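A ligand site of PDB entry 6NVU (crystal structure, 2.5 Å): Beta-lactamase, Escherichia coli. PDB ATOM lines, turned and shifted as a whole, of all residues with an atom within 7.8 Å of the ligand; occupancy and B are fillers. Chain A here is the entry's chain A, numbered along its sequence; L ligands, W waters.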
ATOM      1  N   THR A   3      -4.387   9.537  15.198  1.00  0.00           N
ATOM      2  CA  THR A   3      -4.271   8.536  16.259  1.00  0.00           C
ATOM      3  C   THR A   3      -2.858   8.442  16.825  1.00  0.00           C
ATOM      4  O   THR A   3      -2.618   7.651  17.737  1.00  0.00           O
ATOM      5  CB  THR A   3      -4.739   7.149  15.754  1.00  0.00           C
ATOM      6  OG1 THR A   3      -4.320   6.142  16.689  1.00  0.00           O
ATOM      7  CG2 THR A   3      -4.171   6.814  14.372  1.00  0.00           C
ATOM      8  N   VAL A  25      -6.265  -0.485  22.732  1.00  0.00           N
ATOM      9  CA  VAL A  25      -7.617  -0.102  22.356  1.00  0.00           C
ATOM     10  C   VAL A  25      -7.947  -0.726  21.018  1.00  0.00           C
ATOM     11  O   VAL A  25      -7.157  -0.648  20.077  1.00  0.00           O
ATOM     12  CB  VAL A  25      -7.782   1.421  22.290  1.00  0.00           C
ATOM     13  CG1 VAL A  25      -9.257   1.783  22.185  1.00  0.00           C
ATOM     14  CG2 VAL A  25      -7.141   2.082  23.491  1.00  0.00           C
ATOM     15  N   LEU A  26      -9.133  -1.328  20.914  1.00  0.00           N
ATOM     16  CA  LEU A  26      -9.590  -1.912  19.666  1.00  0.00           C
ATOM     17  C   LEU A  26     -11.026  -1.470  19.431  1.00  0.00           C
ATOM     18  O   LEU A  26     -11.886  -1.695  20.285  1.00  0.00           O
ATOM     19  CB  LEU A  26      -9.498  -3.430  19.697  1.00  0.00           C
ATOM     20  CG  LEU A  26      -8.985  -4.168  18.469  1.00  0.00           C
ATOM     21  CD1 LEU A  26      -7.794  -3.465  17.908  1.00  0.00           C
ATOM     22  CD2 LEU A  26      -8.645  -5.606  18.828  1.00  0.00           C
ATOM     23  N   GLY A  27     -11.264  -0.797  18.309  1.00  0.00           N
ATOM     24  CA  GLY A  27     -12.623  -0.505  17.925  1.00  0.00           C
ATOM     25  C   GLY A  27     -13.408  -1.789  17.710  1.00  0.00           C
ATOM     26  O   GLY A  27     -12.875  -2.803  17.252  1.00  0.00           O
ATOM     27  N   ILE A  28     -14.691  -1.755  18.064  1.00  0.00           N
ATOM     28  CA  ILE A  28     -15.563  -2.895  17.834  1.00  0.00           C
ATOM     29  C   ILE A  28     -16.127  -2.812  16.417  1.00  0.00           C
ATOM     30  O   ILE A  28     -15.863  -3.682  15.589  1.00  0.00           O
ATOM     31  CB  ILE A  28     -16.697  -2.954  18.886  1.00  0.00           C
ATOM     32  CG1 ILE A  28     -16.103  -3.083  20.282  1.00  0.00           C
ATOM     33  CG2 ILE A  28     -17.611  -4.136  18.609  1.00  0.00           C
ATOM     34  CD1 ILE A  28     -15.079  -4.197  20.404  1.00  0.00           C
ATOM     35  N   GLU A  29     -16.897  -1.760  16.141  1.00  0.00           N
ATOM     36  CA  GLU A  29     -17.537  -1.611  14.835  1.00  0.00           C
ATOM     37  C   GLU A  29     -16.549  -1.108  13.795  1.00  0.00           C
ATOM     38  O   GLU A  29     -16.489  -1.625  12.677  1.00  0.00           O
ATOM     39  CB  GLU A  29     -18.730  -0.673  14.944  1.00  0.00           C
ATOM     40  CG  GLU A  29     -19.785  -1.111  15.910  1.00  0.00           C
ATOM     41  CD  GLU A  29     -19.468  -0.774  17.342  1.00  0.00           C
ATOM     42  OE1 GLU A  29     -18.532   0.009  17.574  1.00  0.00           O
ATOM     43  OE2 GLU A  29     -20.152  -1.311  18.240  1.00  0.00           O
ATOM     44  N   ASP A  30     -15.797  -0.076  14.133  1.00  0.00           N
ATOM     45  CA  ASP A  30     -14.780   0.465  13.253  1.00  0.00           C
ATOM     46  C   ASP A  30     -13.411  -0.056  13.660  1.00  0.00           C
ATOM     47  O   ASP A  30     -13.193  -0.410  14.820  1.00  0.00           O
ATOM     48  CB  ASP A  30     -14.800   1.995  13.271  1.00  0.00           C
ATOM     49  CG  ASP A  30     -16.127   2.549  12.765  1.00  0.00           C
ATOM     50  OD1 ASP A  30     -16.904   1.751  12.191  1.00  0.00           O
ATOM     51  OD2 ASP A  30     -16.396   3.768  12.919  1.00  0.00           O
ATOM     52  N   ASN A  31     -12.496  -0.105  12.704  1.00  0.00           N
ATOM     53  CA  ASN A  31     -11.233  -0.808  12.895  1.00  0.00           C
ATOM     54  C   ASN A  31     -10.137   0.151  13.378  1.00  0.00           C
ATOM     55  O   ASN A  31      -9.137   0.412  12.707  1.00  0.00           O
ATOM     56  CB  ASN A  31     -10.824  -1.518  11.620  1.00  0.00           C
ATOM     57  CG  ASN A  31     -10.152  -2.848  11.895  1.00  0.00           C
ATOM     58  OD1 ASN A  31      -9.329  -2.949  12.809  1.00  0.00           O
ATOM     59  ND2 ASN A  31     -10.511  -3.880  11.129  1.00  0.00           N
ATOM     60  N   PHE A  32     -10.330   0.632  14.600  1.00  0.00           N
ATOM     61  CA  PHE A  32      -9.411   1.534  15.279  1.00  0.00           C
ATOM     62  C   PHE A  32      -8.489   0.739  16.193  1.00  0.00           C
ATOM     63  O   PHE A  32      -8.932  -0.194  16.867  1.00  0.00           O
ATOM     64  CB  PHE A  32     -10.183   2.569  16.085  1.00  0.00           C
ATOM     65  CG  PHE A  32      -9.341   3.349  17.041  1.00  0.00           C
ATOM     66  CD1 PHE A  32      -9.122   2.897  18.323  1.00  0.00           C
ATOM     67  CD2 PHE A  32      -8.751   4.533  16.644  1.00  0.00           C
ATOM     68  CE1 PHE A  32      -8.333   3.609  19.206  1.00  0.00           C
ATOM     69  CE2 PHE A  32      -7.963   5.259  17.510  1.00  0.00           C
ATOM     70  CZ  PHE A  32      -7.753   4.785  18.799  1.00  0.00           C
ATOM     71  N   LYS A  33      -7.218   1.129  16.246  1.00  0.00           N
ATOM     72  CA  LYS A  33      -6.237   0.385  17.023  1.00  0.00           C
ATOM     73  C   LYS A  33      -5.289   1.357  17.714  1.00  0.00           C
ATOM     74  O   LYS A  33      -4.994   2.437  17.194  1.00  0.00           O
ATOM     75  CB  LYS A  33      -5.464  -0.588  16.117  1.00  0.00           C
ATOM     76  CG  LYS A  33      -4.424  -1.453  16.802  1.00  0.00           C
ATOM     77  CD  LYS A  33      -4.013  -2.631  15.899  1.00  0.00           C
ATOM     78  CE  LYS A  33      -2.504  -2.928  15.944  1.00  0.00           C
ATOM     79  NZ  LYS A  33      -2.127  -3.878  17.038  1.00  0.00           N
ATOM     80  N   ILE A 235     -16.668  -0.387  26.230  1.00  0.00           N
ATOM     81  CA  ILE A 235     -17.300   0.890  26.545  1.00  0.00           C
ATOM     82  C   ILE A 235     -18.173   1.350  25.383  1.00  0.00           C
ATOM     83  O   ILE A 235     -17.800   1.201  24.208  1.00  0.00           O
ATOM     84  CB  ILE A 235     -16.238   1.961  26.880  1.00  0.00           C
ATOM     85  CG1 ILE A 235     -15.345   1.457  28.011  1.00  0.00           C
ATOM     86  CG2 ILE A 235     -16.881   3.301  27.230  1.00  0.00           C
ATOM     87  CD1 ILE A 235     -14.372   2.436  28.477  1.00  0.00           C
ATOM     88  N   LEU A 237     -19.839   4.365  23.270  1.00  0.00           N
ATOM     89  CA  LEU A 237     -19.647   5.750  22.893  1.00  0.00           C
ATOM     90  C   LEU A 237     -20.990   6.442  22.695  1.00  0.00           C
ATOM     91  O   LEU A 237     -22.002   5.782  22.453  1.00  0.00           O
ATOM     92  CB  LEU A 237     -18.818   5.830  21.611  1.00  0.00           C
ATOM     93  CG  LEU A 237     -17.340   5.484  21.781  1.00  0.00           C
ATOM     94  CD1 LEU A 237     -16.719   4.940  20.474  1.00  0.00           C
ATOM     95  CD2 LEU A 237     -16.570   6.704  22.343  1.00  0.00           C
ATOM     96  N   ASN A 239     -22.376   7.957  20.265  1.00  0.00           N
ATOM     97  CA  ASN A 239     -23.021   7.581  19.023  1.00  0.00           C
ATOM     98  C   ASN A 239     -23.457   6.116  18.980  1.00  0.00           C
ATOM     99  O   ASN A 239     -23.916   5.643  17.929  1.00  0.00           O
ATOM    100  CB  ASN A 239     -22.084   7.886  17.852  1.00  0.00           C
ATOM    101  CG  ASN A 239     -20.918   6.921  17.770  1.00  0.00           C
ATOM    102  OD1 ASN A 239     -20.669   6.112  18.668  1.00  0.00           O
ATOM    103  ND2 ASN A 239     -20.198   7.001  16.670  1.00  0.00           N
ATOM    104  N   GLY A 240     -23.278   5.365  20.079  1.00  0.00           N
ATOM    105  CA  GLY A 240     -23.752   3.992  20.130  1.00  0.00           C
ATOM    106  C   GLY A 240     -22.754   2.931  19.711  1.00  0.00           C
ATOM    107  O   GLY A 240     -23.061   1.742  19.830  1.00  0.00           O
ATOM    108  N   LYS A 241     -21.577   3.322  19.219  1.00  0.00           N
ATOM    109  CA  LYS A 241     -20.527   2.364  18.900  1.00  0.00           C
ATOM    110  C   LYS A 241     -19.807   1.935  20.182  1.00  0.00           C
ATOM    111  O   LYS A 241     -20.079   2.441  21.282  1.00  0.00           O
ATOM    112  CB  LYS A 241     -19.572   2.976  17.875  1.00  0.00           C
ATOM    113  CG  LYS A 241     -20.109   2.865  16.456  1.00  0.00           C
ATOM    114  CD  LYS A 241     -19.444   3.830  15.516  1.00  0.00           C
ATOM    115  CE  LYS A 241     -20.324   4.108  14.295  1.00  0.00           C
ATOM    116  NZ  LYS A 241     -19.783   3.452  13.073  1.00  0.00           N
ATOM    117  N   HIS A 242     -18.884   0.981  20.069  1.00  0.00           N
ATOM    118  CA  HIS A 242     -18.160   0.486  21.234  1.00  0.00           C
ATOM    119  C   HIS A 242     -16.669   0.371  20.950  1.00  0.00           C
ATOM    120  O   HIS A 242     -16.251   0.145  19.807  1.00  0.00           O
ATOM    121  CB  HIS A 242     -18.691  -0.885  21.648  1.00  0.00           C
ATOM    122  CG  HIS A 242     -20.173  -0.919  21.818  1.00  0.00           C
ATOM    123  ND1 HIS A 242     -21.041  -0.960  20.755  1.00  0.00           N
ATOM    124  CD2 HIS A 242     -20.947  -0.881  22.937  1.00  0.00           C
ATOM    125  CE1 HIS A 242     -22.286  -0.965  21.201  1.00  0.00           C
ATOM    126  NE2 HIS A 242     -22.255  -0.918  22.520  1.00  0.00           N
ATOM    127  N   PHE A 243     -15.854   0.473  22.010  1.00  0.00           N
ATOM    128  CA  PHE A 243     -14.452   0.110  21.915  1.00  0.00           C
ATOM    129  C   PHE A 243     -14.013  -0.727  23.110  1.00  0.00           C
ATOM    130  O   PHE A 243     -14.452  -0.499  24.245  1.00  0.00           O
ATOM    131  CB  PHE A 243     -13.525   1.327  21.788  1.00  0.00           C
ATOM    132  CG  PHE A 243     -13.536   2.247  22.988  1.00  0.00           C
ATOM    133  CD1 PHE A 243     -14.563   3.163  23.173  1.00  0.00           C
ATOM    134  CD2 PHE A 243     -12.485   2.213  23.900  1.00  0.00           C
ATOM    135  CE1 PHE A 243     -14.560   4.036  24.259  1.00  0.00           C
ATOM    136  CE2 PHE A 243     -12.469   3.073  25.002  1.00  0.00           C
ATOM    137  CZ  PHE A 243     -13.507   3.988  25.188  1.00  0.00           C
ATOM    138  N   ALA A 244     -13.149  -1.710  22.841  1.00  0.00           N
ATOM    139  CA  ALA A 244     -12.491  -2.495  23.868  1.00  0.00           C
ATOM    140  C   ALA A 244     -11.179  -1.829  24.263  1.00  0.00           C
ATOM    141  O   ALA A 244     -10.451  -1.286  23.435  1.00  0.00           O
ATOM    142  CB  ALA A 244     -12.245  -3.920  23.385  1.00  0.00           C
ATOM    143  N   VAL A 270      -8.622   8.529  25.502  1.00  0.00           N
ATOM    144  CA  VAL A 270      -9.090   7.708  24.399  1.00  0.00           C
ATOM    145  C   VAL A 270     -10.563   8.002  24.136  1.00  0.00           C
ATOM    146  O   VAL A 270     -10.982   8.127  22.973  1.00  0.00           O
ATOM    147  CB  VAL A 270      -8.842   6.218  24.702  1.00  0.00           C
ATOM    148  CG1 VAL A 270      -9.446   5.318  23.622  1.00  0.00           C
ATOM    149  CG2 VAL A 270      -7.347   5.946  24.865  1.00  0.00           C
ATOM    150  N   ASP A 272     -12.100  10.780  24.546  1.00  0.00           N
ATOM    151  CA  ASP A 272     -12.262  12.069  23.897  1.00  0.00           C
ATOM    152  C   ASP A 272     -11.871  12.003  22.431  1.00  0.00           C
ATOM    153  O   ASP A 272     -12.481  12.668  21.591  1.00  0.00           O
ATOM    154  CB  ASP A 272     -11.448  13.146  24.610  1.00  0.00           C
ATOM    155  CG  ASP A 272     -11.976  13.455  25.973  1.00  0.00           C
ATOM    156  OD1 ASP A 272     -13.056  12.922  26.327  1.00  0.00           O
ATOM    157  OD2 ASP A 272     -11.320  14.238  26.696  1.00  0.00           O
ATOM    158  N   TYR A 273     -10.847  11.209  22.108  1.00  0.00           N
ATOM    159  CA  TYR A 273     -10.418  11.106  20.724  1.00  0.00           C
ATOM    160  C   TYR A 273     -11.510  10.482  19.871  1.00  0.00           C
ATOM    161  O   TYR A 273     -11.888  11.013  18.822  1.00  0.00           O
ATOM    162  CB  TYR A 273      -9.110  10.312  20.627  1.00  0.00           C
ATOM    163  CG  TYR A 273      -8.677  10.053  19.210  1.00  0.00           C
ATOM    164  CD1 TYR A 273      -8.104  11.070  18.441  1.00  0.00           C
ATOM    165  CD2 TYR A 273      -8.866   8.823  18.625  1.00  0.00           C
ATOM    166  CE1 TYR A 273      -7.716  10.847  17.137  1.00  0.00           C
ATOM    167  CE2 TYR A 273      -8.478   8.590  17.318  1.00  0.00           C
ATOM    168  CZ  TYR A 273      -7.912   9.601  16.580  1.00  0.00           C
ATOM    169  OH  TYR A 273      -7.544   9.347  15.271  1.00  0.00           O
ATOM    170  N   LEU A 274     -12.068   9.356  20.339  1.00  0.00           N
ATOM    171  CA  LEU A 274     -13.090   8.641  19.584  1.00  0.00           C
ATOM    172  C   LEU A 274     -14.424   9.367  19.566  1.00  0.00           C
ATOM    173  O   LEU A 274     -15.233   9.120  18.660  1.00  0.00           O
ATOM    174  CB  LEU A 274     -13.249   7.236  20.159  1.00  0.00           C
ATOM    175  CG  LEU A 274     -11.995   6.370  20.102  1.00  0.00           C
ATOM    176  CD1 LEU A 274     -12.223   5.020  20.745  1.00  0.00           C
ATOM    177  CD2 LEU A 274     -11.557   6.196  18.671  1.00  0.00           C
ATOM    178  N   VAL A 275     -14.670  10.262  20.521  1.00  0.00           N
ATOM    179  CA  VAL A 275     -15.923  10.998  20.510  1.00  0.00           C
ATOM    180  C   VAL A 275     -15.955  11.992  19.349  1.00  0.00           C
ATOM    181  O   VAL A 275     -17.014  12.286  18.800  1.00  0.00           O
ATOM    182  CB  VAL A 275     -16.163  11.650  21.884  1.00  0.00           C
ATOM    183  CG1 VAL A 275     -17.001  12.889  21.775  1.00  0.00           C
ATOM    184  CG2 VAL A 275     -16.838  10.668  22.810  1.00  0.00           C
ATOM    185  N   LYS A 276     -14.788  12.490  18.931  1.00  0.00           N
ATOM    186  CA  LYS A 276     -14.635  13.195  17.655  1.00  0.00           C
ATOM    187  C   LYS A 276     -14.564  12.157  16.539  1.00  0.00           C
ATOM    188  O   LYS A 276     -13.491  11.641  16.210  1.00  0.00           O
ATOM    189  CB  LYS A 276     -13.394  14.069  17.690  1.00  0.00           C
ATOM    190  CG  LYS A 276     -13.076  14.599  19.080  1.00  0.00           C
ATOM    191  CD  LYS A 276     -12.320  15.919  19.029  1.00  0.00           C
ATOM    192  CE  LYS A 276     -10.960  15.746  18.373  1.00  0.00           C
ATOM    193  NZ  LYS A 276     -10.534  16.987  17.642  1.00  0.00           N
ATOM    194  N   ASP A 277     -15.724  11.878  15.928  1.00  0.00           N
ATOM    195  CA  ASP A 277     -15.963  10.788  14.966  1.00  0.00           C
ATOM    196  C   ASP A 277     -14.969   9.630  15.050  1.00  0.00           C
ATOM    197  O   ASP A 277     -14.425   9.198  14.029  1.00  0.00           O
ATOM    198  CB  ASP A 277     -15.984  11.330  13.525  1.00  0.00           C
ATOM    199  CG  ASP A 277     -14.684  12.051  13.134  1.00  0.00           C
ATOM    200  OD1 ASP A 277     -13.604  11.736  13.687  1.00  0.00           O
ATOM    201  OD2 ASP A 277     -14.755  12.926  12.238  1.00  0.00           O
HETATM  202  O1  LIG L   1     -12.384   7.974  15.889  1.00  0.00           O
HETATM  203  C1  LIG L   1     -12.630   6.887  15.441  1.00  0.00           C
HETATM  204  C2  LIG L   1     -11.845   5.655  15.032  1.00  0.00           C
HETATM  205  C3  LIG L   1     -13.243   5.028  14.733  1.00  0.00           C
HETATM  206  N1  LIG L   1     -13.851   6.301  15.117  1.00  0.00           N
HETATM  207  O2  LIG L   1     -13.645   4.044  15.701  1.00  0.00           O
HETATM  208  C4  LIG L   1     -14.661   4.564  16.447  1.00  0.00           C
HETATM  209  C5  LIG L   1     -14.922   6.007  16.074  1.00  0.00           C
HETATM  210  C6  LIG L   1     -16.273   6.146  15.401  1.00  0.00           C
HETATM  211  O3  LIG L   1     -17.275   6.179  16.083  1.00  0.00           O
HETATM  212  O4  LIG L   1     -16.302   6.228  14.201  1.00  0.00           O
HETATM  213  C7  LIG L   1     -15.343   3.766  17.372  1.00  0.00           C
HETATM  214  C8  LIG L   1     -14.941   2.326  17.603  1.00  0.00           C
HETATM  215  O5  LIG L   1     -15.821   1.453  16.938  1.00  0.00           O
HETATM  216  O   HOH W   1     -17.717   8.210  17.968  1.00  0.00           O
HETATM  217  O   HOH W   2     -19.192   7.218  14.145  1.00  0.00           O
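N of Asp 30 lies within hydrogen-bond range of O5 of the ligand.
OD2 of Asp 30 lies close to O4 of the ligand (2.8 Å).
O3 of the ligand is in hydrogen-bond range of ND2 of Asn 239, 3.1 Å away.
An oxygen (O5) of the ligand lies within hydrogen-bond range of the backbone NH (N) of Glu 29 (3.5 Å).
An oxygen (O5) of the ligand sits at hydrogen-bond distance from the side-chain carboxylate (OE1) of Glu 29 (3.1 Å).
O of His 242 lies within hydrogen-bond range of O5 of the ligand, at 3.2 Å.
The side-chain amino group of Lys 241 lies within salt-bridge range of the side-chain carboxylate of Asp 30, 3.4 Å away.
OD1 of Asn 239 is in hydrogen-bond range of N of Lys 241, 3.0 Å away.
ND1 of His 242 is in hydrogen-bond range of OE2 of Glu 29 (2.7 Å).
The backbone carbonyl oxygen (O) of His 242 sits at hydrogen-bond distance from the backbone NH (N) of Ile 28, 3.0 Å away.
O of Gly 240 sits close to ND1 of His 242 (3.5 Å).
The backbone carbonyl oxygen (O) of Phe 32 sits at hydrogen-bond distance from the backbone NH (N) of Gly 27 (2.8 Å).
An oxygen (O1) of the ligand lies close to the backbone carbonyl oxygen (O) of Asp 277 (3.0 Å).
Residues that only touch the ligand: Gly 27, Ile 28, Phe 32, Leu 237, Lys 241, Leu 274 and Lys 276.
12 residues have an atom within 4 Å of the ligand: Gly 27, Ile 28, Glu 29, Asp 30, Phe 32, Leu 237, Asn 239, Lys 241, His 242, Leu 274, Lys 276 and Asp 277.
Along chain A the residues within 4 Å of the ligand span positions 27 to 277.
Water W1 lies within hydrogen-bond range of the backbone carbonyl oxygen of Leu 274 (2.7 Å), an oxygen (O3) of the ligand (2.8 Å) and the side-chain amide nitrogen of Asn 239 (3.0 Å).
Water W2 bridges ND2 of Asn 239 (2.7 Å) and O3 of the ligand (2.9 Å).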
